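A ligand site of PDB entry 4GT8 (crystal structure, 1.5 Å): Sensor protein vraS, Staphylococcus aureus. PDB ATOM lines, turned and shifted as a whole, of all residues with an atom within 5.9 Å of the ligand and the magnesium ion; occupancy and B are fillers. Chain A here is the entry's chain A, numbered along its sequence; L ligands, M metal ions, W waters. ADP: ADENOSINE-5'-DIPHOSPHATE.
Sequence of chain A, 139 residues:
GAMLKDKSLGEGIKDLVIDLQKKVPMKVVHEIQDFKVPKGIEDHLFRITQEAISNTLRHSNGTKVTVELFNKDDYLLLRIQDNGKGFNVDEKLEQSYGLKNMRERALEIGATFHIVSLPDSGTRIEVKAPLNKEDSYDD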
ATOM      1  N   GLU A  51       4.484  25.069  29.623  1.00  0.00           N
ATOM      2  CA  GLU A  51       4.481  24.383  28.331  1.00  0.00           C
ATOM      3  C   GLU A  51       3.289  24.803  27.458  1.00  0.00           C
ATOM      4  O   GLU A  51       3.442  25.047  26.258  1.00  0.00           O
ATOM      5  CB  GLU A  51       4.500  22.873  28.528  1.00  0.00           C
ATOM      6  CG  GLU A  51       4.392  22.074  27.240  1.00  0.00           C
ATOM      7  CD  GLU A  51       5.554  22.328  26.291  1.00  0.00           C
ATOM      8  OE1 GLU A  51       6.635  22.775  26.749  1.00  0.00           O
ATOM      9  OE2 GLU A  51       5.389  22.072  25.084  1.00  0.00           O
ATOM     10  N   ALA A  52       2.121  24.896  28.068  1.00  0.00           N
ATOM     11  CA  ALA A  52       0.935  25.304  27.350  1.00  0.00           C
ATOM     12  C   ALA A  52       1.111  26.705  26.767  1.00  0.00           C
ATOM     13  O   ALA A  52       0.777  26.956  25.596  1.00  0.00           O
ATOM     14  CB  ALA A  52      -0.293  25.241  28.271  1.00  0.00           C
ATOM     15  N   SER A  54       4.042  28.215  26.143  1.00  0.00           N
ATOM     16  CA  SER A  54       5.098  28.091  25.145  1.00  0.00           C
ATOM     17  C   SER A  54       4.548  27.635  23.799  1.00  0.00           C
ATOM     18  O   SER A  54       4.891  28.175  22.745  1.00  0.00           O
ATOM     19  CB  SER A  54       6.181  27.116  25.620  1.00  0.00           C
ATOM     20  OG  SER A  54       7.068  26.816  24.551  1.00  0.00           O
ATOM     21  N   ASN A  55       3.703  26.613  23.826  1.00  0.00           N
ATOM     22  CA  ASN A  55       3.138  26.080  22.597  1.00  0.00           C
ATOM     23  C   ASN A  55       2.212  27.073  21.913  1.00  0.00           C
ATOM     24  O   ASN A  55       2.204  27.193  20.685  1.00  0.00           O
ATOM     25  CB  ASN A  55       2.388  24.796  22.875  1.00  0.00           C
ATOM     26  CG  ASN A  55       3.308  23.651  23.180  1.00  0.00           C
ATOM     27  OD1 ASN A  55       4.503  23.699  22.889  1.00  0.00           O
ATOM     28  ND2 ASN A  55       2.743  22.582  23.739  1.00  0.00           N
ATOM     29  N   THR A  56       1.401  27.785  22.696  1.00  0.00           N
ATOM     30  CA  THR A  56       0.534  28.803  22.134  1.00  0.00           C
ATOM     31  C   THR A  56       1.343  29.898  21.433  1.00  0.00           C
ATOM     32  O   THR A  56       1.047  30.269  20.295  1.00  0.00           O
ATOM     33  CB  THR A  56      -0.369  29.391  23.223  1.00  0.00           C
ATOM     34  OG1 THR A  56      -1.402  28.454  23.545  1.00  0.00           O
ATOM     35  CG2 THR A  56      -1.012  30.626  22.721  1.00  0.00           C
ATOM     36  N   ARG A  58       4.437  29.840  20.271  1.00  0.00           N
ATOM     37  CA  ARG A  58       5.187  29.370  19.113  1.00  0.00           C
ATOM     38  C   ARG A  58       4.334  28.891  17.952  1.00  0.00           C
ATOM     39  O   ARG A  58       4.693  29.101  16.794  1.00  0.00           O
ATOM     40  CB  ARG A  58       6.151  28.256  19.508  1.00  0.00           C
ATOM     41  CG  ARG A  58       7.286  28.054  18.521  1.00  0.00           C
ATOM     42  CD  ARG A  58       8.220  26.928  18.963  1.00  0.00           C
ATOM     43  NE  ARG A  58       8.670  27.113  20.342  1.00  0.00           N
ATOM     44  CZ  ARG A  58       9.004  26.109  21.158  1.00  0.00           C
ATOM     45  NH1 ARG A  58       8.922  24.860  20.741  1.00  0.00           N
ATOM     46  NH2 ARG A  58       9.401  26.376  22.399  1.00  0.00           N
ATOM     47  N   HIS A  59       3.214  28.230  18.259  1.00  0.00           N
ATOM     48  CA  HIS A  59       2.502  27.429  17.265  1.00  0.00           C
ATOM     49  C   HIS A  59       1.121  27.956  16.829  1.00  0.00           C
ATOM     50  O   HIS A  59       0.649  27.615  15.748  1.00  0.00           O
ATOM     51  CB  HIS A  59       2.290  25.993  17.763  1.00  0.00           C
ATOM     52  CG  HIS A  59       3.542  25.286  18.190  1.00  0.00           C
ATOM     53  ND1 HIS A  59       4.590  25.026  17.336  1.00  0.00           N
ATOM     54  CD2 HIS A  59       3.877  24.731  19.381  1.00  0.00           C
ATOM     55  CE1 HIS A  59       5.529  24.362  17.987  1.00  0.00           C
ATOM     56  NE2 HIS A  59       5.121  24.172  19.228  1.00  0.00           N
ATOM     57  N   SER A  60       0.457  28.743  17.668  1.00  0.00           N
ATOM     58  CA  SER A  60      -0.957  29.055  17.406  1.00  0.00           C
ATOM     59  C   SER A  60      -1.192  30.128  16.355  1.00  0.00           C
ATOM     60  O   SER A  60      -2.210  30.096  15.668  1.00  0.00           O
ATOM     61  CB  SER A  60      -1.695  29.427  18.701  1.00  0.00           C
ATOM     62  OG  SER A  60      -1.382  30.746  19.115  1.00  0.00           O
ATOM     63  N   ASP A  82      -6.184  29.374  23.772  1.00  0.00           N
ATOM     64  CA  ASP A  82      -5.801  30.360  22.766  1.00  0.00           C
ATOM     65  C   ASP A  82      -6.840  30.455  21.654  1.00  0.00           C
ATOM     66  O   ASP A  82      -7.663  29.567  21.495  1.00  0.00           O
ATOM     67  CB  ASP A  82      -4.373  30.133  22.239  1.00  0.00           C
ATOM     68  CG  ASP A  82      -4.244  28.922  21.311  1.00  0.00           C
ATOM     69  OD1 ASP A  82      -4.995  28.809  20.325  1.00  0.00           O
ATOM     70  OD2 ASP A  82      -3.337  28.087  21.540  1.00  0.00           O
ATOM     71  N   LYS A  85      -4.865  28.761  15.521  1.00  0.00           N
ATOM     72  CA  LYS A  85      -5.223  27.942  14.370  1.00  0.00           C
ATOM     73  C   LYS A  85      -5.680  26.524  14.705  1.00  0.00           C
ATOM     74  O   LYS A  85      -6.305  25.854  13.883  1.00  0.00           O
ATOM     75  CB  LYS A  85      -4.028  27.875  13.400  1.00  0.00           C
ATOM     76  CG  LYS A  85      -2.805  27.170  13.963  1.00  0.00           C
ATOM     77  CD  LYS A  85      -1.559  27.457  13.149  1.00  0.00           C
ATOM     78  CE  LYS A  85      -1.634  26.883  11.754  1.00  0.00           C
ATOM     79  NZ  LYS A  85      -0.445  27.274  10.945  1.00  0.00           N
ATOM     80  N   GLY A  86      -5.366  26.070  15.911  1.00  0.00           N
ATOM     81  CA  GLY A  86      -5.705  24.716  16.311  1.00  0.00           C
ATOM     82  C   GLY A  86      -4.804  23.689  15.653  1.00  0.00           C
ATOM     83  O   GLY A  86      -4.025  24.015  14.757  1.00  0.00           O
ATOM     84  N   PHE A  87      -4.915  22.448  16.118  1.00  0.00           N
ATOM     85  CA  PHE A  87      -4.159  21.334  15.546  1.00  0.00           C
ATOM     86  C   PHE A  87      -4.865  20.031  15.861  1.00  0.00           C
ATOM     87  O   PHE A  87      -5.785  19.988  16.685  1.00  0.00           O
ATOM     88  CB  PHE A  87      -2.699  21.310  16.016  1.00  0.00           C
ATOM     89  CG  PHE A  87      -2.506  20.900  17.464  1.00  0.00           C
ATOM     90  CD1 PHE A  87      -2.805  21.777  18.494  1.00  0.00           C
ATOM     91  CD2 PHE A  87      -2.027  19.641  17.791  1.00  0.00           C
ATOM     92  CE1 PHE A  87      -2.613  21.413  19.816  1.00  0.00           C
ATOM     93  CE2 PHE A  87      -1.854  19.264  19.104  1.00  0.00           C
ATOM     94  CZ  PHE A  87      -2.152  20.152  20.126  1.00  0.00           C
ATOM     95  N   LYS A  92      -0.307  14.411  16.520  1.00  0.00           N
ATOM     96  CA  LYS A  92       0.923  14.862  17.175  1.00  0.00           C
ATOM     97  C   LYS A  92       1.281  14.091  18.447  1.00  0.00           C
ATOM     98  O   LYS A  92       2.464  13.860  18.726  1.00  0.00           O
ATOM     99  CB  LYS A  92       0.830  16.354  17.525  1.00  0.00           C
ATOM    100  CG  LYS A  92       0.458  17.269  16.378  1.00  0.00           C
ATOM    101  CD  LYS A  92       1.556  17.350  15.337  1.00  0.00           C
ATOM    102  CE  LYS A  92       1.254  18.443  14.316  1.00  0.00           C
ATOM    103  NZ  LYS A  92       2.286  18.511  13.252  1.00  0.00           N
ATOM    104  N   SER A  96       5.162  13.641  20.353  1.00  0.00           N
ATOM    105  CA  SER A  96       5.340  15.002  20.873  1.00  0.00           C
ATOM    106  C   SER A  96       5.732  15.030  22.346  1.00  0.00           C
ATOM    107  O   SER A  96       4.953  14.636  23.211  1.00  0.00           O
ATOM    108  CB  SER A  96       4.054  15.793  20.675  1.00  0.00           C
ATOM    109  OG  SER A  96       3.667  15.784  19.313  1.00  0.00           O
ATOM    110  N   TYR A  97       6.925  15.533  22.654  1.00  0.00           N
ATOM    111  CA  TYR A  97       7.401  15.454  24.023  1.00  0.00           C
ATOM    112  C   TYR A  97       6.729  16.468  24.947  1.00  0.00           C
ATOM    113  O   TYR A  97       6.533  16.191  26.132  1.00  0.00           O
ATOM    114  CB  TYR A  97       8.925  15.608  24.085  1.00  0.00           C
ATOM    115  CG  TYR A  97       9.651  14.477  23.418  1.00  0.00           C
ATOM    116  CD1 TYR A  97       9.955  13.318  24.118  1.00  0.00           C
ATOM    117  CD2 TYR A  97      10.031  14.563  22.090  1.00  0.00           C
ATOM    118  CE1 TYR A  97      10.622  12.271  23.516  1.00  0.00           C
ATOM    119  CE2 TYR A  97      10.701  13.522  21.472  1.00  0.00           C
ATOM    120  CZ  TYR A  97      10.992  12.379  22.183  1.00  0.00           C
ATOM    121  OH  TYR A  97      11.659  11.331  21.581  1.00  0.00           O
ATOM    122  N   GLY A  98       6.407  17.641  24.404  1.00  0.00           N
ATOM    123  CA  GLY A  98       5.709  18.660  25.172  1.00  0.00           C
ATOM    124  C   GLY A  98       4.340  18.197  25.662  1.00  0.00           C
ATOM    125  O   GLY A  98       4.011  18.317  26.840  1.00  0.00           O
ATOM    126  N   LEU A  99       3.544  17.644  24.756  1.00  0.00           N
ATOM    127  CA  LEU A  99       2.214  17.174  25.128  1.00  0.00           C
ATOM    128  C   LEU A  99       2.333  16.002  26.098  1.00  0.00           C
ATOM    129  O   LEU A  99       1.620  15.959  27.114  1.00  0.00           O
ATOM    130  CB  LEU A  99       1.443  16.761  23.886  1.00  0.00           C
ATOM    131  CG  LEU A  99       1.276  17.844  22.812  1.00  0.00           C
ATOM    132  CD1 LEU A  99       0.424  17.312  21.672  1.00  0.00           C
ATOM    133  CD2 LEU A  99       0.682  19.141  23.375  1.00  0.00           C
ATOM    134  N   LYS A 100       3.219  15.062  25.781  1.00  0.00           N
ATOM    135  CA  LYS A 100       3.437  13.902  26.651  1.00  0.00           C
ATOM    136  C   LYS A 100       3.873  14.312  28.043  1.00  0.00           C
ATOM    137  O   LYS A 100       3.400  13.764  29.028  1.00  0.00           O
ATOM    138  CB  LYS A 100       4.460  12.953  26.027  1.00  0.00           C
ATOM    139  CG  LYS A 100       3.865  12.072  24.933  1.00  0.00           C
ATOM    140  CD  LYS A 100       4.812  10.940  24.535  1.00  0.00           C
ATOM    141  CE  LYS A 100       5.991  11.463  23.737  1.00  0.00           C
ATOM    142  NZ  LYS A 100       6.934  10.375  23.371  1.00  0.00           N
ATOM    143  N   MET A 102       3.216  17.272  29.633  1.00  0.00           N
ATOM    144  CA  MET A 102       2.088  17.855  30.336  1.00  0.00           C
ATOM    145  C   MET A 102       1.184  16.756  30.868  1.00  0.00           C
ATOM    146  O   MET A 102       0.724  16.820  32.008  1.00  0.00           O
ATOM    147  CB  MET A 102       1.282  18.793  29.417  1.00  0.00           C
ATOM    148  CG  MET A 102       1.966  20.154  29.170  1.00  0.00           C
ATOM    149  SD  MET A 102       0.909  21.337  28.306  1.00  0.00           S
ATOM    150  CE  MET A 102       0.873  20.586  26.682  1.00  0.00           C
ATOM    151  N   SER A 117      -8.892  20.910  20.563  1.00  0.00           N
ATOM    152  CA  SER A 117      -8.326  21.735  19.503  1.00  0.00           C
ATOM    153  C   SER A 117      -9.024  21.416  18.199  1.00  0.00           C
ATOM    154  O   SER A 117      -8.883  20.318  17.640  1.00  0.00           O
ATOM    155  CB  SER A 117      -6.827  21.486  19.385  1.00  0.00           C
ATOM    156  OG  SER A 117      -6.213  22.530  18.637  1.00  0.00           O
ATOM    157  N   THR A 123      -7.010  26.348  20.561  1.00  0.00           N
ATOM    158  CA  THR A 123      -6.564  25.224  21.400  1.00  0.00           C
ATOM    159  C   THR A 123      -6.853  25.487  22.863  1.00  0.00           C
ATOM    160  O   THR A 123      -6.466  26.525  23.401  1.00  0.00           O
ATOM    161  CB  THR A 123      -5.061  24.967  21.228  1.00  0.00           C
ATOM    162  OG1 THR A 123      -4.797  24.602  19.869  1.00  0.00           O
ATOM    163  CG2 THR A 123      -4.572  23.849  22.171  1.00  0.00           C
HETATM  164  PB  ADP L   1       7.008  21.323  20.358  1.00  0.00           P
HETATM  165  O1B ADP L   1       8.352  20.778  20.806  1.00  0.00           O
HETATM  166  O2B ADP L   1       6.882  21.486  18.864  1.00  0.00           O
HETATM  167  O3B ADP L   1       6.570  22.517  21.174  1.00  0.00           O
HETATM  168  PA  ADP L   1       4.798  19.863  21.611  1.00  0.00           P
HETATM  169  O1A ADP L   1       4.825  18.423  22.082  1.00  0.00           O
HETATM  170  O2A ADP L   1       4.785  20.937  22.657  1.00  0.00           O
HETATM  171  O3A ADP L   1       5.980  20.072  20.550  1.00  0.00           O
HETATM  172  O5' ADP L   1       3.559  20.062  20.597  1.00  0.00           O
HETATM  173  C5' ADP L   1       3.471  19.195  19.467  1.00  0.00           C
HETATM  174  C4' ADP L   1       2.885  19.894  18.249  1.00  0.00           C
HETATM  175  O4' ADP L   1       1.517  20.230  18.457  1.00  0.00           O
HETATM  176  C3' ADP L   1       3.556  21.221  17.946  1.00  0.00           C
HETATM  177  O3' ADP L   1       4.738  21.056  17.167  1.00  0.00           O
HETATM  178  C2' ADP L   1       2.478  21.960  17.185  1.00  0.00           C
HETATM  179  O2' ADP L   1       2.432  21.491  15.841  1.00  0.00           O
HETATM  180  C1' ADP L   1       1.202  21.462  17.807  1.00  0.00           C
HETATM  181  N9  ADP L   1       0.686  22.410  18.828  1.00  0.00           N
HETATM  182  C8  ADP L   1       0.861  22.301  20.156  1.00  0.00           C
HETATM  183  N7  ADP L   1       0.221  23.291  20.801  1.00  0.00           N
HETATM  184  C5  ADP L   1      -0.376  24.069  19.870  1.00  0.00           C
HETATM  185  C6  ADP L   1      -1.210  25.268  19.895  1.00  0.00           C
HETATM  186  N6  ADP L   1      -1.526  25.868  21.056  1.00  0.00           N
HETATM  187  N1  ADP L   1      -1.661  25.737  18.713  1.00  0.00           N
HETATM  188  C2  ADP L   1      -1.343  25.144  17.536  1.00  0.00           C
HETATM  189  N3  ADP L   1      -0.578  24.039  17.446  1.00  0.00           N
HETATM  190  C4  ADP L   1      -0.082  23.473  18.568  1.00  0.00           C
HETATM  191 MG    MG M   1       6.014  22.350  23.159  1.00  0.00          MG
HETATM  192  O   HOH W   1      -0.201  22.740  23.657  1.00  0.00           O
HETATM  193  O   HOH W   2      10.593  22.237  21.802  1.00  0.00           O
HETATM  194  O   HOH W   3       7.138  23.937  23.898  1.00  0.00           O
HETATM  195  O   HOH W   4      -1.246  25.408  24.086  1.00  0.00           O
HETATM  196  O   HOH W   5       8.303  19.546  17.079  1.00  0.00           O
HETATM  197  O   HOH W   6       0.369  23.406  14.931  1.00  0.00           O
HETATM  198  O   HOH W   7       7.605  21.071  23.528  1.00  0.00           O
HETATM  199  O   HOH W   8       4.551  22.395  14.280  1.00  0.00           O
HETATM  200  O   HOH W   9      -4.198  26.837  18.519  1.00  0.00           O
HETATM  201  O   HOH W  10       7.994  17.913  21.199  1.00  0.00           O
HETATM  202  O   HOH W  11       4.887  18.971  15.288  1.00  0.00           O
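N6 of the ligand is in hydrogen-bond range of OD2 of Asp 82. N of Gly 98 is in hydrogen-bond range of O1A of the ligand (2.9 Å). An oxygen (O2B) of the ligand lies within hydrogen-bond range of a ring nitrogen (NE2) of His 59, 3.2 Å away. An oxygen (O1A) of the ligand is in hydrogen-bond range of the backbone NH of Leu 99. NH1 of Arg 58 sits close to O3B of the ligand (3.3 Å).
The backbone carbonyl oxygen (O) of Thr 123 sits at hydrogen-bond distance from the backbone NH (N) of Asp 82. The side-chain hydroxyl of Thr 56 lies within hydrogen-bond range of the side-chain carboxylate of Asp 82 (2.8 Å). OG of Ser 117 sits at hydrogen-bond distance from N of Phe 87, at 2.8 Å. NH2 of Arg 58 sits at hydrogen-bond distance from OG of Ser 54, at 3.2 Å. The side-chain hydroxyl (OG1) of Thr 123 is in hydrogen-bond range of the side-chain hydroxyl (OG) of Ser 117 (2.8 Å). O of Thr 56 is in hydrogen-bond range of OG of Ser 60, at 2.7 Å. O of Ala 52 is in hydrogen-bond range of OG1 of Thr 56. The backbone carbonyl oxygen of Ser 60 sits at hydrogen-bond distance from the backbone NH of Lys 85 (3.0 Å).
Merely in contact with the ligand: Thr 56, Ser 60, Phe 87, Lys 92, Ser 96, Tyr 97 and Thr 123. Of the 21 residues printed, 14 come within 4 Å of the ligand. The nearest printed residue that does not touch the ligand is Gly 86 (4.02 Å).
The magnesium ion is bound by an oxygen (O2A) of the ligand, 1.9 Å away. OD1 of Asn 55 is bound to the magnesium ion. The magnesium ion is bound by the side-chain carboxylate (OE2) of Glu 51 (2.0 Å). The magnesium ion is bound by O3B of the ligand, 2.1 Å away. The magnesium ion is bound by water W7 (2.1 Å). Water W3 binds the magnesium ion (2.1 Å). The magnesium ion has six donor atoms within binding distance.
Water W3 lies within hydrogen-bond range of OG of Ser 54 and OE1 of Glu 51. Water W9 lies within hydrogen-bond range of the side-chain hydroxyl (OG1) of Thr 123 (2.7 Å), a nitrogen (N1) of the ligand (2.8 Å), the side-chain carboxylate (OD1) of Asp 82 (2.8 Å) and the backbone NH (N) of Gly 86 (3.0 Å). Water W11 bridges an oxygen (O3') of the ligand (2.8 Å) and the side-chain amino group (NZ) of Lys 92 (3.3 Å). Water W2 lies within hydrogen-bond range of an oxygen (O1B) of the ligand (2.9 Å) and the guanidinium group (NH1) of Arg 58 (3.3 Å). Water W1 bridges a nitrogen (N7) of the ligand (2.9 Å) and the side-chain amide nitrogen of Asn 55 (2.9 Å). Water W4 lies within hydrogen-bond range of the backbone carbonyl oxygen (O) of Ala 52, a nitrogen (N6) of the ligand and the side-chain hydroxyl (OG1) of Thr 56.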
